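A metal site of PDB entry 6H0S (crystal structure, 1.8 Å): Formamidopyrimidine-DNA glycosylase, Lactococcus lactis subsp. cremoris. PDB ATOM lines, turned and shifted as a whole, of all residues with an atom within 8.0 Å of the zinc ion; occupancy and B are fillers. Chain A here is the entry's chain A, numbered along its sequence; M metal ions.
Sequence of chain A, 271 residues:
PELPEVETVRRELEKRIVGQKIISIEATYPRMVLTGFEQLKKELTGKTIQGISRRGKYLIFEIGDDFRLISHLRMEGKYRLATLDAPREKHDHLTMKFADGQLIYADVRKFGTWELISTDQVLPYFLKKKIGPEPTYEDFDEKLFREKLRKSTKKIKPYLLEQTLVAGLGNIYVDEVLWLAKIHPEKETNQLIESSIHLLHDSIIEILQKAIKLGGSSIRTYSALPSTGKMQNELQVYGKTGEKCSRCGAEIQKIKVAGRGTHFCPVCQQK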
ATOM      1  N   TRP A 179     -22.039 -14.467 -10.848  1.00  0.00           N
ATOM      2  CA  TRP A 179     -23.215 -13.997 -10.101  1.00  0.00           C
ATOM      3  C   TRP A 179     -22.781 -13.342  -8.783  1.00  0.00           C
ATOM      4  O   TRP A 179     -23.282 -12.264  -8.407  1.00  0.00           O
ATOM      5  CB  TRP A 179     -24.165 -15.171  -9.824  1.00  0.00           C
ATOM      6  CG  TRP A 179     -25.392 -14.770  -8.986  1.00  0.00           C
ATOM      7  CD1 TRP A 179     -26.599 -14.307  -9.448  1.00  0.00           C
ATOM      8  CD2 TRP A 179     -25.498 -14.798  -7.561  1.00  0.00           C
ATOM      9  NE1 TRP A 179     -27.440 -14.055  -8.387  1.00  0.00           N
ATOM     10  CE2 TRP A 179     -26.788 -14.364  -7.226  1.00  0.00           C
ATOM     11  CE3 TRP A 179     -24.621 -15.185  -6.536  1.00  0.00           C
ATOM     12  CZ2 TRP A 179     -27.239 -14.284  -5.895  1.00  0.00           C
ATOM     13  CZ3 TRP A 179     -25.057 -15.089  -5.215  1.00  0.00           C
ATOM     14  CH2 TRP A 179     -26.356 -14.644  -4.906  1.00  0.00           C
ATOM     15  N   LYS A 182     -21.395  -9.991  -9.403  1.00  0.00           N
ATOM     16  CA  LYS A 182     -22.309  -9.086 -10.071  1.00  0.00           C
ATOM     17  C   LYS A 182     -21.785  -8.620 -11.428  1.00  0.00           C
ATOM     18  O   LYS A 182     -21.923  -7.458 -11.798  1.00  0.00           O
ATOM     19  CB  LYS A 182     -22.663  -7.894  -9.169  1.00  0.00           C
ATOM     20  CG  LYS A 182     -23.353  -8.421  -7.861  1.00  0.00           C
ATOM     21  CD  LYS A 182     -23.814  -7.209  -7.004  1.00  0.00           C
ATOM     22  CE  LYS A 182     -24.413  -7.617  -5.676  1.00  0.00           C
ATOM     23  NZ  LYS A 182     -25.456  -6.640  -5.223  1.00  0.00           N
ATOM     24  N   VAL A 237     -27.043 -19.993  -9.144  1.00  0.00           N
ATOM     25  CA  VAL A 237     -27.520 -19.775 -10.510  1.00  0.00           C
ATOM     26  C   VAL A 237     -27.390 -21.012 -11.399  1.00  0.00           C
ATOM     27  O   VAL A 237     -28.239 -21.253 -12.262  1.00  0.00           O
ATOM     28  CB  VAL A 237     -26.805 -18.594 -11.183  1.00  0.00           C
ATOM     29  CG1 VAL A 237     -27.299 -17.260 -10.582  1.00  0.00           C
ATOM     30  CG2 VAL A 237     -25.257 -18.691 -11.081  1.00  0.00           C
ATOM     31  N   LYS A 244     -35.882 -17.996  -8.632  1.00  0.00           N
ATOM     32  CA  LYS A 244     -35.659 -16.588  -8.331  1.00  0.00           C
ATOM     33  C   LYS A 244     -34.288 -16.370  -7.719  1.00  0.00           C
ATOM     34  O   LYS A 244     -33.821 -17.183  -6.910  1.00  0.00           O
ATOM     35  CB  LYS A 244     -36.748 -16.043  -7.398  1.00  0.00           C
ATOM     36  CG  LYS A 244     -38.204 -16.347  -7.834  1.00  0.00           C
ATOM     37  CD  LYS A 244     -38.605 -15.808  -9.224  1.00  0.00           C
ATOM     38  CE  LYS A 244     -40.072 -16.171  -9.579  1.00  0.00           C
ATOM     39  NZ  LYS A 244     -40.576 -15.785 -10.954  1.00  0.00           N
ATOM     40  N   CYS A 245     -33.616 -15.295  -8.148  1.00  0.00           N
ATOM     41  CA  CYS A 245     -32.348 -14.853  -7.573  1.00  0.00           C
ATOM     42  C   CYS A 245     -32.492 -14.637  -6.073  1.00  0.00           C
ATOM     43  O   CYS A 245     -33.427 -13.979  -5.615  1.00  0.00           O
ATOM     44  CB  CYS A 245     -31.932 -13.554  -8.249  1.00  0.00           C
ATOM     45  SG  CYS A 245     -30.465 -12.791  -7.557  1.00  0.00           S
ATOM     46  N   SER A 246     -31.575 -15.199  -5.289  1.00  0.00           N
ATOM     47  CA  SER A 246     -31.679 -15.051  -3.832  1.00  0.00           C
ATOM     48  C   SER A 246     -31.441 -13.629  -3.347  1.00  0.00           C
ATOM     49  O   SER A 246     -31.752 -13.340  -2.192  1.00  0.00           O
ATOM     50  CB  SER A 246     -30.690 -15.973  -3.152  1.00  0.00           C
ATOM     51  OG  SER A 246     -29.376 -15.506  -3.408  1.00  0.00           O
ATOM     52  N   ARG A 247     -30.897 -12.741  -4.181  1.00  0.00           N
ATOM     53  CA  ARG A 247     -30.622 -11.363  -3.785  1.00  0.00           C
ATOM     54  C   ARG A 247     -31.758 -10.431  -4.135  1.00  0.00           C
ATOM     55  O   ARG A 247     -32.215  -9.677  -3.274  1.00  0.00           O
ATOM     56  CB  ARG A 247     -29.308 -10.847  -4.411  1.00  0.00           C
ATOM     57  CG  ARG A 247     -28.054 -11.231  -3.644  1.00  0.00           C
ATOM     58  CD  ARG A 247     -26.739 -10.588  -4.237  1.00  0.00           C
ATOM     59  NE  ARG A 247     -26.664 -10.821  -5.663  1.00  0.00           N
ATOM     60  CZ  ARG A 247     -25.561 -11.133  -6.338  1.00  0.00           C
ATOM     61  NH1 ARG A 247     -24.390 -11.234  -5.716  1.00  0.00           N
ATOM     62  NH2 ARG A 247     -25.637 -11.322  -7.646  1.00  0.00           N
ATOM     63  N   CYS A 248     -32.253 -10.470  -5.378  1.00  0.00           N
ATOM     64  CA  CYS A 248     -33.231  -9.500  -5.846  1.00  0.00           C
ATOM     65  C   CYS A 248     -34.582 -10.073  -6.220  1.00  0.00           C
ATOM     66  O   CYS A 248     -35.497  -9.292  -6.450  1.00  0.00           O
ATOM     67  CB  CYS A 248     -32.704  -8.731  -7.071  1.00  0.00           C
ATOM     68  SG  CYS A 248     -32.569  -9.743  -8.551  1.00  0.00           S
ATOM     69  N   GLY A 249     -34.721 -11.407  -6.322  1.00  0.00           N
ATOM     70  CA  GLY A 249     -35.971 -12.033  -6.652  1.00  0.00           C
ATOM     71  C   GLY A 249     -36.300 -12.103  -8.128  1.00  0.00           C
ATOM     72  O   GLY A 249     -37.368 -12.602  -8.489  1.00  0.00           O
ATOM     73  N   ALA A 250     -35.433 -11.613  -8.998  1.00  0.00           N
ATOM     74  CA  ALA A 250     -35.635 -11.777 -10.434  1.00  0.00           C
ATOM     75  C   ALA A 250     -35.414 -13.236 -10.833  1.00  0.00           C
ATOM     76  O   ALA A 250     -34.617 -13.929 -10.213  1.00  0.00           O
ATOM     77  CB  ALA A 250     -34.668 -10.873 -11.203  1.00  0.00           C
ATOM     78  N   GLU A 251     -36.084 -13.667 -11.912  1.00  0.00           N
ATOM     79  CA  GLU A 251     -35.883 -15.030 -12.411  1.00  0.00           C
ATOM     80  C   GLU A 251     -34.507 -15.197 -13.026  1.00  0.00           C
ATOM     81  O   GLU A 251     -34.102 -14.394 -13.882  1.00  0.00           O
ATOM     82  CB  GLU A 251     -36.908 -15.419 -13.473  1.00  0.00           C
ATOM     83  CG  GLU A 251     -38.024 -16.136 -12.890  1.00  0.00           C
ATOM     84  CD  GLU A 251     -39.017 -16.673 -13.868  1.00  0.00           C
ATOM     85  OE1 GLU A 251     -38.754 -17.063 -15.027  1.00  0.00           O
ATOM     86  OE2 GLU A 251     -40.137 -16.752 -13.393  1.00  0.00           O
ATOM     87  N   ILE A 252     -33.805 -16.260 -12.628  1.00  0.00           N
ATOM     88  CA  ILE A 252     -32.554 -16.627 -13.286  1.00  0.00           C
ATOM     89  C   ILE A 252     -32.818 -16.991 -14.743  1.00  0.00           C
ATOM     90  O   ILE A 252     -33.733 -17.761 -15.070  1.00  0.00           O
ATOM     91  CB  ILE A 252     -31.868 -17.784 -12.545  1.00  0.00           C
ATOM     92  CG1 ILE A 252     -31.541 -17.389 -11.097  1.00  0.00           C
ATOM     93  CG2 ILE A 252     -30.636 -18.277 -13.311  1.00  0.00           C
ATOM     94  CD1 ILE A 252     -30.848 -16.013 -10.954  1.00  0.00           C
ATOM     95  N   PHE A 264     -27.575 -16.692 -15.309  1.00  0.00           N
ATOM     96  CA  PHE A 264     -27.224 -15.429 -14.658  1.00  0.00           C
ATOM     97  C   PHE A 264     -28.495 -14.741 -14.184  1.00  0.00           C
ATOM     98  O   PHE A 264     -29.594 -15.052 -14.645  1.00  0.00           O
ATOM     99  CB  PHE A 264     -26.459 -14.504 -15.634  1.00  0.00           C
ATOM    100  CG  PHE A 264     -27.338 -13.965 -16.740  1.00  0.00           C
ATOM    101  CD1 PHE A 264     -27.761 -14.807 -17.777  1.00  0.00           C
ATOM    102  CD2 PHE A 264     -27.779 -12.647 -16.728  1.00  0.00           C
ATOM    103  CE1 PHE A 264     -28.611 -14.359 -18.773  1.00  0.00           C
ATOM    104  CE2 PHE A 264     -28.624 -12.175 -17.738  1.00  0.00           C
ATOM    105  CZ  PHE A 264     -29.044 -13.045 -18.765  1.00  0.00           C
ATOM    106  N   CYS A 265     -28.352 -13.781 -13.272  1.00  0.00           N
ATOM    107  CA  CYS A 265     -29.459 -12.903 -12.897  1.00  0.00           C
ATOM    108  C   CYS A 265     -29.392 -11.620 -13.710  1.00  0.00           C
ATOM    109  O   CYS A 265     -28.394 -10.908 -13.622  1.00  0.00           O
ATOM    110  CB  CYS A 265     -29.422 -12.564 -11.406  1.00  0.00           C
ATOM    111  SG  CYS A 265     -30.684 -11.303 -11.003  1.00  0.00           S
ATOM    112  N   PRO A 266     -30.428 -11.272 -14.490  1.00  0.00           N
ATOM    113  CA  PRO A 266     -30.369 -10.064 -15.333  1.00  0.00           C
ATOM    114  C   PRO A 266     -30.395  -8.763 -14.567  1.00  0.00           C
ATOM    115  O   PRO A 266     -30.087  -7.725 -15.160  1.00  0.00           O
ATOM    116  CB  PRO A 266     -31.631 -10.157 -16.204  1.00  0.00           C
ATOM    117  CG  PRO A 266     -32.111 -11.536 -16.011  1.00  0.00           C
ATOM    118  CD  PRO A 266     -31.676 -12.013 -14.687  1.00  0.00           C
ATOM    119  N   VAL A 267     -30.817  -8.788 -13.305  1.00  0.00           N
ATOM    120  CA  VAL A 267     -30.817  -7.564 -12.490  1.00  0.00           C
ATOM    121  C   VAL A 267     -29.448  -7.349 -11.856  1.00  0.00           C
ATOM    122  O   VAL A 267     -28.867  -6.257 -11.936  1.00  0.00           O
ATOM    123  CB  VAL A 267     -31.907  -7.650 -11.398  1.00  0.00           C
ATOM    124  CG1 VAL A 267     -31.754  -6.495 -10.393  1.00  0.00           C
ATOM    125  CG2 VAL A 267     -33.283  -7.587 -12.046  1.00  0.00           C
ATOM    126  N   CYS A 268     -28.956  -8.384 -11.188  1.00  0.00           N
ATOM    127  CA  CYS A 268     -27.701  -8.295 -10.454  1.00  0.00           C
ATOM    128  C   CYS A 268     -26.491  -8.246 -11.397  1.00  0.00           C
ATOM    129  O   CYS A 268     -25.437  -7.745 -10.997  1.00  0.00           O
ATOM    130  CB  CYS A 268     -27.551  -9.495  -9.508  1.00  0.00           C
ATOM    131  SG  CYS A 268     -28.710  -9.537  -8.097  1.00  0.00           S
ATOM    132  N   GLN A 269     -26.619  -8.787 -12.613  1.00  0.00           N
ATOM    133  CA  GLN A 269     -25.506  -8.905 -13.561  1.00  0.00           C
ATOM    134  C   GLN A 269     -25.891  -8.103 -14.783  1.00  0.00           C
ATOM    135  O   GLN A 269     -26.376  -8.640 -15.778  1.00  0.00           O
ATOM    136  CB  GLN A 269     -25.180 -10.371 -13.908  1.00  0.00           C
ATOM    137  CG  GLN A 269     -24.736 -11.150 -12.697  1.00  0.00           C
ATOM    138  CD  GLN A 269     -24.763 -12.653 -12.948  1.00  0.00           C
ATOM    139  OE1 GLN A 269     -25.701 -13.329 -12.559  1.00  0.00           O
ATOM    140  NE2 GLN A 269     -23.701 -13.179 -13.576  1.00  0.00           N
HETATM  141 ZN    ZN M   1     -30.530 -10.816  -8.743  1.00  0.00          ZN
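The side-chain sulfur (SG) of Cys 245 lies close to the indole nitrogen (NE1) of Trp 179. The side-chain sulfur (SG) of Cys 245 lies close to the backbone NH (N) of Arg 247, at 3.4 Å. The backbone NH (N) of Cys 245 sits at hydrogen-bond distance from the backbone carbonyl oxygen (O) of Ala 250 (2.7 Å). SG of Cys 248 lies close to N of Ala 250, at 3.4 Å. NE of Arg 247 sits close to SG of Cys 268. The side-chain sulfur (SG) of Cys 265 lies close to the backbone NH (N) of Val 267 (3.4 Å). The backbone NH (N) of Cys 265 is in hydrogen-bond range of the side-chain amide oxygen (OE1) of Gln 269 (2.8 Å).
Within 4 Å of the zinc ion: Cys 245, Cys 248, Cys 265 and Cys 268.
The zinc ion is bound by the side-chain sulfur (SG) of Cys 245 (2.3 Å), the side-chain sulfur (SG) of Cys 248 (2.3 Å), the side-chain sulfur (SG) of Cys 268 (2.3 Å) and the side-chain sulfur (SG) of Cys 265 (2.3 Å).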
